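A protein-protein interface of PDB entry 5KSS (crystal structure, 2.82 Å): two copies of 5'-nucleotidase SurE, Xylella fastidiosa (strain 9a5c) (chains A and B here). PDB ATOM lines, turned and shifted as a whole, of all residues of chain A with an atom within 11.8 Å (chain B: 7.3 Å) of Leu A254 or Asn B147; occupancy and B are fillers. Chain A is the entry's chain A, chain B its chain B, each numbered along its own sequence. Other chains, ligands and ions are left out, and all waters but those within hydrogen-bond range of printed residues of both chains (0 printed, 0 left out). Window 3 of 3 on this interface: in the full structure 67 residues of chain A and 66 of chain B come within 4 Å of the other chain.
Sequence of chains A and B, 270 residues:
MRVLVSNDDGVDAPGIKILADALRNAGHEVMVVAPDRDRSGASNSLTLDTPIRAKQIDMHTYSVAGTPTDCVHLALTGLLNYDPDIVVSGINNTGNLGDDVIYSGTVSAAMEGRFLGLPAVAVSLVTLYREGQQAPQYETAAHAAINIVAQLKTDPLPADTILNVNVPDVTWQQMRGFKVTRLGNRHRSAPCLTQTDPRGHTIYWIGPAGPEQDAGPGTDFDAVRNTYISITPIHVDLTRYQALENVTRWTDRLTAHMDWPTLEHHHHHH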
ATOM      1  N   ASN A 246      -2.446   4.881  -2.271  1.00  0.00           N
ATOM      2  CA  ASN A 246      -2.783   5.845  -3.314  1.00  0.00           C
ATOM      3  C   ASN A 246      -1.809   7.021  -3.378  1.00  0.00           C
ATOM      4  O   ASN A 246      -1.375   7.419  -4.459  1.00  0.00           O
ATOM      5  CB  ASN A 246      -4.213   6.357  -3.120  1.00  0.00           C
ATOM      6  CG  ASN A 246      -4.679   7.231  -4.268  1.00  0.00           C
ATOM      7  N   VAL A 247      -1.472   7.570  -2.214  1.00  0.00           N
ATOM      8  CA  VAL A 247      -0.579   8.723  -2.120  1.00  0.00           C
ATOM      9  C   VAL A 247       0.820   8.393  -2.645  1.00  0.00           C
ATOM     10  O   VAL A 247       1.494   9.247  -3.222  1.00  0.00           O
ATOM     11  CB  VAL A 247      -0.489   9.242  -0.666  1.00  0.00           C
ATOM     12  CG1 VAL A 247       0.392  10.479  -0.586  1.00  0.00           C
ATOM     13  CG2 VAL A 247      -1.876   9.548  -0.128  1.00  0.00           C
ATOM     14  N   THR A 248       1.240   7.147  -2.452  1.00  0.00           N
ATOM     15  CA  THR A 248       2.546   6.691  -2.920  1.00  0.00           C
ATOM     16  C   THR A 248       2.668   6.802  -4.437  1.00  0.00           C
ATOM     17  O   THR A 248       3.693   7.247  -4.957  1.00  0.00           O
ATOM     18  CB  THR A 248       2.828   5.242  -2.481  1.00  0.00           C
ATOM     19  OG1 THR A 248       2.737   5.148  -1.053  1.00  0.00           O
ATOM     20  CG2 THR A 248       4.218   4.809  -2.923  1.00  0.00           C
ATOM     21  N   ARG A 249       1.617   6.397  -5.144  1.00  0.00           N
ATOM     22  CA  ARG A 249       1.570   6.535  -6.595  1.00  0.00           C
ATOM     23  C   ARG A 249       1.529   8.010  -6.970  1.00  0.00           C
ATOM     24  O   ARG A 249       2.138   8.433  -7.954  1.00  0.00           O
ATOM     25  CB  ARG A 249       0.335   5.836  -7.161  1.00  0.00           C
ATOM     26  CG  ARG A 249       0.209   4.371  -6.788  1.00  0.00           C
ATOM     27  CD  ARG A 249      -1.065   3.784  -7.373  1.00  0.00           C
ATOM     28  NE  ARG A 249      -1.220   2.368  -7.050  1.00  0.00           N
ATOM     29  CZ  ARG A 249      -1.948   1.911  -6.036  1.00  0.00           C
ATOM     30  NH1 ARG A 249      -2.591   2.757  -5.244  1.00  0.00           N
ATOM     31  NH2 ARG A 249      -2.033   0.606  -5.817  1.00  0.00           N
ATOM     32  N   TRP A 250       0.797   8.785  -6.176  1.00  0.00           N
ATOM     33  CA  TRP A 250       0.665  10.219  -6.394  1.00  0.00           C
ATOM     34  C   TRP A 250       1.994  10.927  -6.160  1.00  0.00           C
ATOM     35  O   TRP A 250       2.323  11.897  -6.842  1.00  0.00           O
ATOM     36  CB  TRP A 250      -0.407  10.795  -5.467  1.00  0.00           C
ATOM     37  CG  TRP A 250      -0.533  12.285  -5.536  1.00  0.00           C
ATOM     38  CD1 TRP A 250      -1.358  13.001  -6.351  1.00  0.00           C
ATOM     39  CD2 TRP A 250       0.190  13.243  -4.754  1.00  0.00           C
ATOM     40  NE1 TRP A 250      -1.194  14.347  -6.128  1.00  0.00           N
ATOM     41  CE2 TRP A 250      -0.249  14.522  -5.153  1.00  0.00           C
ATOM     42  CE3 TRP A 250       1.167  13.145  -3.759  1.00  0.00           C
ATOM     43  CZ2 TRP A 250       0.256  15.692  -4.589  1.00  0.00           C
ATOM     44  CZ3 TRP A 250       1.665  14.307  -3.201  1.00  0.00           C
ATOM     45  CH2 TRP A 250       1.208  15.565  -3.618  1.00  0.00           C
ATOM     46  N   THR A 251       2.753  10.430  -5.188  1.00  0.00           N
ATOM     47  CA  THR A 251       4.038  11.020  -4.835  1.00  0.00           C
ATOM     48  C   THR A 251       5.112  10.655  -5.857  1.00  0.00           C
ATOM     49  O   THR A 251       5.962  11.479  -6.199  1.00  0.00           O
ATOM     50  CB  THR A 251       4.474  10.587  -3.421  1.00  0.00           C
ATOM     51  OG1 THR A 251       3.542  11.098  -2.459  1.00  0.00           O
ATOM     52  CG2 THR A 251       5.856  11.116  -3.096  1.00  0.00           C
ATOM     53  N   ASP A 252       5.064   9.420  -6.348  1.00  0.00           N
ATOM     54  CA  ASP A 252       6.007   8.965  -7.365  1.00  0.00           C
ATOM     55  C   ASP A 252       5.847   9.750  -8.663  1.00  0.00           C
ATOM     56  O   ASP A 252       6.830  10.041  -9.346  1.00  0.00           O
ATOM     57  CB  ASP A 252       5.846   7.465  -7.627  1.00  0.00           C
ATOM     58  CG  ASP A 252       6.400   6.616  -6.500  1.00  0.00           C
ATOM     59  OD1 ASP A 252       7.331   7.079  -5.808  1.00  0.00           O
ATOM     60  OD2 ASP A 252       5.909   5.483  -6.306  1.00  0.00           O
ATOM     61  N   ARG A 253       4.608  10.097  -8.996  1.00  0.00           N
ATOM     62  CA  ARG A 253       4.336  10.922 -10.168  1.00  0.00           C
ATOM     63  C   ARG A 253       4.760  12.367  -9.922  1.00  0.00           C
ATOM     64  O   ARG A 253       4.809  13.178 -10.848  1.00  0.00           O
ATOM     65  CB  ARG A 253       2.854  10.859 -10.547  1.00  0.00           C
ATOM     66  N   LEU A 254       5.064  12.680  -8.666  1.00  0.00           N
ATOM     67  CA  LEU A 254       5.531  14.009  -8.290  1.00  0.00           C
ATOM     68  C   LEU A 254       7.034  13.995  -8.019  1.00  0.00           C
ATOM     69  O   LEU A 254       7.711  15.014  -8.161  1.00  0.00           O
ATOM     70  CB  LEU A 254       4.775  14.510  -7.056  1.00  0.00           C
ATOM     71  CG  LEU A 254       5.121  15.909  -6.543  1.00  0.00           C
ATOM     72  CD1 LEU A 254       4.861  16.958  -7.615  1.00  0.00           C
ATOM     73  CD2 LEU A 254       4.342  16.225  -5.276  1.00  0.00           C
ATOM     74  N   THR A 255       7.550  12.832  -7.632  1.00  0.00           N
ATOM     75  CA  THR A 255       8.971  12.680  -7.340  1.00  0.00           C
ATOM     76  C   THR A 255       9.816  12.831  -8.601  1.00  0.00           C
ATOM     77  O   THR A 255      10.287  13.924  -8.918  1.00  0.00           O
ATOM     78  CB  THR A 255       9.276  11.315  -6.692  1.00  0.00           C
ATOM     79  OG1 THR A 255       8.534  11.183  -5.471  1.00  0.00           O
ATOM     80  CG2 THR A 255      10.760  11.187  -6.391  1.00  0.00           C
ATOM     81  N   LEU B  23       3.218  30.769  -3.363  1.00  0.00           N
ATOM     82  CA  LEU B  23       1.969  30.375  -4.004  1.00  0.00           C
ATOM     83  C   LEU B  23       1.451  31.475  -4.926  1.00  0.00           C
ATOM     84  O   LEU B  23       0.821  31.193  -5.945  1.00  0.00           O
ATOM     85  CB  LEU B  23       0.917  30.010  -2.956  1.00  0.00           C
ATOM     86  CG  LEU B  23       1.203  28.750  -2.136  1.00  0.00           C
ATOM     87  CD1 LEU B  23       0.164  28.568  -1.042  1.00  0.00           C
ATOM     88  CD2 LEU B  23       1.252  27.527  -3.038  1.00  0.00           C
ATOM     89  N   ALA B  26       3.435  31.267  -7.992  1.00  0.00           N
ATOM     90  CA  ALA B  26       3.153  30.007  -8.670  1.00  0.00           C
ATOM     91  C   ALA B  26       1.880  30.094  -9.508  1.00  0.00           C
ATOM     92  O   ALA B  26       1.496  29.131 -10.172  1.00  0.00           O
ATOM     93  CB  ALA B  26       3.053  28.871  -7.665  1.00  0.00           C
ATOM     94  N   HIS B  28      -1.130  30.884  -8.207  1.00  0.00           N
ATOM     95  CA  HIS B  28      -2.281  30.517  -7.392  1.00  0.00           C
ATOM     96  C   HIS B  28      -2.867  31.738  -6.693  1.00  0.00           C
ATOM     97  O   HIS B  28      -2.132  32.593  -6.202  1.00  0.00           O
ATOM     98  CB  HIS B  28      -1.893  29.464  -6.351  1.00  0.00           C
ATOM     99  CG  HIS B  28      -1.377  28.189  -6.941  1.00  0.00           C
ATOM    100  ND1 HIS B  28      -2.204  27.243  -7.506  1.00  0.00           N
ATOM    101  CD2 HIS B  28      -0.119  27.700  -7.046  1.00  0.00           C
ATOM    102  CE1 HIS B  28      -1.478  26.228  -7.939  1.00  0.00           C
ATOM    103  NE2 HIS B  28      -0.209  26.481  -7.671  1.00  0.00           N
ATOM    104  N   THR B 140      12.564  26.393   0.977  1.00  0.00           N
ATOM    105  CA  THR B 140      12.588  24.990   0.584  1.00  0.00           C
ATOM    106  C   THR B 140      11.246  24.330   0.880  1.00  0.00           C
ATOM    107  O   THR B 140      10.731  23.554   0.074  1.00  0.00           O
ATOM    108  CB  THR B 140      13.701  24.222   1.319  1.00  0.00           C
ATOM    109  OG1 THR B 140      14.964  24.855   1.075  1.00  0.00           O
ATOM    110  CG2 THR B 140      13.763  22.780   0.838  1.00  0.00           C
ATOM    111  N   ALA B 141      10.683  24.649   2.041  1.00  0.00           N
ATOM    112  CA  ALA B 141       9.388  24.108   2.436  1.00  0.00           C
ATOM    113  C   ALA B 141       8.277  24.671   1.558  1.00  0.00           C
ATOM    114  O   ALA B 141       7.312  23.976   1.237  1.00  0.00           O
ATOM    115  CB  ALA B 141       9.114  24.405   3.902  1.00  0.00           C
ATOM    116  N   ALA B 142       8.420  25.933   1.170  1.00  0.00           N
ATOM    117  CA  ALA B 142       7.454  26.577   0.290  1.00  0.00           C
ATOM    118  C   ALA B 142       7.552  26.010  -1.120  1.00  0.00           C
ATOM    119  O   ALA B 142       6.537  25.765  -1.773  1.00  0.00           O
ATOM    120  CB  ALA B 142       7.669  28.081   0.278  1.00  0.00           C
ATOM    121  N   HIS B 143       8.783  25.801  -1.580  1.00  0.00           N
ATOM    122  CA  HIS B 143       9.031  25.235  -2.902  1.00  0.00           C
ATOM    123  C   HIS B 143       8.442  23.833  -2.998  1.00  0.00           C
ATOM    124  O   HIS B 143       7.975  23.413  -4.055  1.00  0.00           O
ATOM    125  CB  HIS B 143      10.533  25.199  -3.194  1.00  0.00           C
ATOM    126  CG  HIS B 143      10.870  24.790  -4.594  1.00  0.00           C
ATOM    127  ND1 HIS B 143      12.125  24.355  -4.958  1.00  0.00           N
ATOM    128  CD2 HIS B 143      10.119  24.759  -5.721  1.00  0.00           C
ATOM    129  CE1 HIS B 143      12.132  24.068  -6.249  1.00  0.00           C
ATOM    130  NE2 HIS B 143      10.928  24.305  -6.734  1.00  0.00           N
ATOM    131  N   ALA B 144       8.469  23.110  -1.885  1.00  0.00           N
ATOM    132  CA  ALA B 144       7.852  21.794  -1.818  1.00  0.00           C
ATOM    133  C   ALA B 144       6.339  21.928  -1.939  1.00  0.00           C
ATOM    134  O   ALA B 144       5.692  21.162  -2.651  1.00  0.00           O
ATOM    135  CB  ALA B 144       8.218  21.107  -0.519  1.00  0.00           C
ATOM    136  N   ALA B 145       5.791  22.917  -1.240  1.00  0.00           N
ATOM    137  CA  ALA B 145       4.350  23.136  -1.202  1.00  0.00           C
ATOM    138  C   ALA B 145       3.766  23.478  -2.570  1.00  0.00           C
ATOM    139  O   ALA B 145       2.714  22.960  -2.947  1.00  0.00           O
ATOM    140  CB  ALA B 145       4.007  24.220  -0.190  1.00  0.00           C
ATOM    141  N   ILE B 146       4.449  24.345  -3.313  1.00  0.00           N
ATOM    142  CA  ILE B 146       3.953  24.785  -4.615  1.00  0.00           C
ATOM    143  C   ILE B 146       3.919  23.649  -5.639  1.00  0.00           C
ATOM    144  O   ILE B 146       3.179  23.713  -6.621  1.00  0.00           O
ATOM    145  CB  ILE B 146       4.764  25.976  -5.176  1.00  0.00           C
ATOM    146  CG1 ILE B 146       6.190  25.548  -5.519  1.00  0.00           C
ATOM    147  CG2 ILE B 146       4.765  27.133  -4.189  1.00  0.00           C
ATOM    148  CD1 ILE B 146       7.057  26.675  -6.037  1.00  0.00           C
ATOM    149  N   ASN B 147       4.717  22.612  -5.403  1.00  0.00           N
ATOM    150  CA  ASN B 147       4.703  21.431  -6.258  1.00  0.00           C
ATOM    151  C   ASN B 147       3.580  20.479  -5.870  1.00  0.00           C
ATOM    152  O   ASN B 147       2.988  19.818  -6.723  1.00  0.00           O
ATOM    153  CB  ASN B 147       6.049  20.703  -6.202  1.00  0.00           C
ATOM    154  CG  ASN B 147       7.160  21.474  -6.888  1.00  0.00           C
ATOM    155  OD1 ASN B 147       7.321  21.401  -8.106  1.00  0.00           O
ATOM    156  ND2 ASN B 147       7.938  22.214  -6.108  1.00  0.00           N
ATOM    157  N   ILE B 148       3.292  20.415  -4.574  1.00  0.00           N
ATOM    158  CA  ILE B 148       2.229  19.559  -4.061  1.00  0.00           C
ATOM    159  C   ILE B 148       0.858  20.058  -4.501  1.00  0.00           C
ATOM    160  O   ILE B 148       0.040  19.286  -5.004  1.00  0.00           O
ATOM    161  CB  ILE B 148       2.274  19.468  -2.523  1.00  0.00           C
ATOM    162  CG1 ILE B 148       3.551  18.756  -2.072  1.00  0.00           C
ATOM    163  CG2 ILE B 148       1.048  18.744  -1.991  1.00  0.00           C
ATOM    164  CD1 ILE B 148       3.707  18.668  -0.572  1.00  0.00           C
ATOM    165  N   VAL B 149       0.615  21.353  -4.317  1.00  0.00           N
ATOM    166  CA  VAL B 149      -0.653  21.955  -4.711  1.00  0.00           C
ATOM    167  C   VAL B 149      -0.873  21.832  -6.221  1.00  0.00           C
ATOM    168  O   VAL B 149      -1.998  21.626  -6.678  1.00  0.00           O
ATOM    169  CB  VAL B 149      -0.758  23.433  -4.248  1.00  0.00           C
ATOM    170  CG1 VAL B 149       0.362  24.275  -4.844  1.00  0.00           C
ATOM    171  CG2 VAL B 149      -2.120  24.016  -4.600  1.00  0.00           C
ATOM    172  N   ALA B 150       0.210  21.929  -6.985  1.00  0.00           N
ATOM    173  CA  ALA B 150       0.141  21.805  -8.436  1.00  0.00           C
ATOM    174  C   ALA B 150      -0.181  20.372  -8.847  1.00  0.00           C
ATOM    175  O   ALA B 150      -0.920  20.142  -9.802  1.00  0.00           O
ATOM    176  CB  ALA B 150       1.448  22.259  -9.069  1.00  0.00           C
ATOM    177  N   GLN B 151       0.380  19.412  -8.118  1.00  0.00           N
ATOM    178  CA  GLN B 151       0.153  18.003  -8.406  1.00  0.00           C
ATOM    179  C   GLN B 151      -1.274  17.602  -8.041  1.00  0.00           C
ATOM    180  O   GLN B 151      -1.835  16.670  -8.617  1.00  0.00           O
ATOM    181  CB  GLN B 151       1.161  17.135  -7.648  1.00  0.00           C
ATOM    182  N   LEU B 152      -1.857  18.317  -7.084  1.00  0.00           N
ATOM    183  CA  LEU B 152      -3.228  18.058  -6.659  1.00  0.00           C
ATOM    184  C   LEU B 152      -4.240  18.653  -7.633  1.00  0.00           C
ATOM    185  O   LEU B 152      -5.437  18.380  -7.542  1.00  0.00           O
ATOM    186  CB  LEU B 152      -3.470  18.600  -5.249  1.00  0.00           C
ATOM    187  CG  LEU B 152      -2.756  17.858  -4.117  1.00  0.00           C
ATOM    188  CD1 LEU B 152      -3.093  18.474  -2.769  1.00  0.00           C
ATOM    189  CD2 LEU B 152      -3.121  16.385  -4.144  1.00  0.00           C
ATOM    190  N   LYS B 153      -3.756  19.471  -8.562  1.00  0.00           N
ATOM    191  CA  LYS B 153      -4.613  20.042  -9.593  1.00  0.00           C
ATOM    192  C   LYS B 153      -4.997  18.968 -10.603  1.00  0.00           C
ATOM    193  O   LYS B 153      -6.165  18.829 -10.965  1.00  0.00           O
ATOM    194  CB  LYS B 153      -3.913  21.205 -10.295  1.00  0.00           C
ATOM    195  N   TRP B 172      17.157  23.076  -1.321  1.00  0.00           N
ATOM    196  CA  TRP B 172      16.439  22.172  -2.216  1.00  0.00           C
ATOM    197  C   TRP B 172      17.381  21.225  -2.956  1.00  0.00           C
ATOM    198  O   TRP B 172      16.968  20.162  -3.424  1.00  0.00           O
ATOM    199  CB  TRP B 172      15.586  22.965  -3.209  1.00  0.00           C
ATOM    200  CG  TRP B 172      14.731  22.102  -4.084  1.00  0.00           C
ATOM    201  CD1 TRP B 172      15.000  21.712  -5.363  1.00  0.00           C
ATOM    202  CD2 TRP B 172      13.470  21.513  -3.741  1.00  0.00           C
ATOM    203  NE1 TRP B 172      13.983  20.920  -5.840  1.00  0.00           N
ATOM    204  CE2 TRP B 172      13.032  20.783  -4.863  1.00  0.00           C
ATOM    205  CE3 TRP B 172      12.668  21.534  -2.596  1.00  0.00           C
ATOM    206  CZ2 TRP B 172      11.830  20.080  -4.874  1.00  0.00           C
ATOM    207  CZ3 TRP B 172      11.473  20.836  -2.608  1.00  0.00           C
ATOM    208  CH2 TRP B 172      11.066  20.118  -3.740  1.00  0.00           C
ATOM    209  N   PHE B 178      10.789  12.703  -2.299  1.00  0.00           N
ATOM    210  CA  PHE B 178       9.709  12.657  -1.322  1.00  0.00           C
ATOM    211  C   PHE B 178       9.458  11.216  -0.890  1.00  0.00           C
ATOM    212  O   PHE B 178       9.621  10.287  -1.681  1.00  0.00           O
ATOM    213  CB  PHE B 178       8.423  13.244  -1.908  1.00  0.00           C
ATOM    214  CG  PHE B 178       8.578  14.627  -2.475  1.00  0.00           C
ATOM    215  CD1 PHE B 178       9.482  15.524  -1.930  1.00  0.00           C
ATOM    216  CD2 PHE B 178       7.813  15.032  -3.556  1.00  0.00           C
ATOM    217  CE1 PHE B 178       9.622  16.793  -2.458  1.00  0.00           C
ATOM    218  CE2 PHE B 178       7.947  16.301  -4.085  1.00  0.00           C
ATOM    219  CZ  PHE B 178       8.852  17.182  -3.534  1.00  0.00           C
ATOM    220  N   ILE B 231       5.765  12.911   3.807  1.00  0.00           N
ATOM    221  CA  ILE B 231       4.360  13.140   3.512  1.00  0.00           C
ATOM    222  C   ILE B 231       3.518  12.064   4.183  1.00  0.00           C
ATOM    223  O   ILE B 231       3.515  10.908   3.758  1.00  0.00           O
ATOM    224  CB  ILE B 231       4.081  13.129   1.998  1.00  0.00           C
ATOM    225  CG1 ILE B 231       4.851  14.253   1.303  1.00  0.00           C
ATOM    226  CG2 ILE B 231       2.592  13.274   1.730  1.00  0.00           C
ATOM    227  CD1 ILE B 231       4.554  14.369  -0.176  1.00  0.00           C
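O of Gln B151 sits at hydrogen-bond distance from NE1 of Trp A250 (3.5 Å).
The backbone carbonyl oxygen of Val A247 lies within hydrogen-bond range of the side-chain hydroxyl of Thr A251, 2.9 Å away. The side-chain hydroxyl (OG1) of Thr A255 lies within hydrogen-bond range of the backbone carbonyl oxygen (O) of Thr A251 (2.7 Å).
Among the printed residues, merely in contact across the chains: Trp A250 with Leu B152, Leu A254 with Asn B147, Thr A251 with Phe B178, Trp A250 with Ile B148, Leu A254 with Gln B151 and Leu A254 with Phe B178.
Val A247 touches none of the printed residues of chain B. Of the printed residues of chain B, Thr A251 touches Phe B178. Of chain B, only Asn B147, Gln B151 and Phe B178 come within 4 Å of Leu A254. No residue of chain A comes within 4 Å of His B143. No residue of chain A comes within 4 Å of Ala B144. No residue of chain A comes within 4 Å of Ala B145. Ile B146 touches none of the printed residues of chain A. Of chain A, only Leu A254 comes within 4 Å of Asn B147. Ile B148 touches one residue of chain A. No residue of chain A comes within 4 Å of Ala B150. Of chain A, only Trp A250 and Leu A254 come within 4 Å of Gln B151. Printed residues of chain A within 4 Å of Leu B152: Trp A250. Printed residues of chain A within 4 Å of Phe B178: Thr A251 and Leu A254. The nearest residue of chain B that does not touch Leu A254 is Ile B148 (4.1 Å). The nearest printed residue of chain A that does not touch Leu B152 is Leu A254 (6.8 Å).
No position is printed for both chains. Of the 7 pairs that touch across the chains among the printed residues, none has its exchanged pair printed and touching as well.
Hydrophobic or aromatic side chains of chain A that line the printed part of chain B: Trp A250 and Leu A254. Hydrophobic or aromatic side chains of chain B that line the printed part of chain A: Ile B148, Leu B152 and Phe B178. Along chain B the printed residues that touch a printed residue of chain A span positions 147 to 178. Among the printed residues, 7 pairs touch across the chains.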
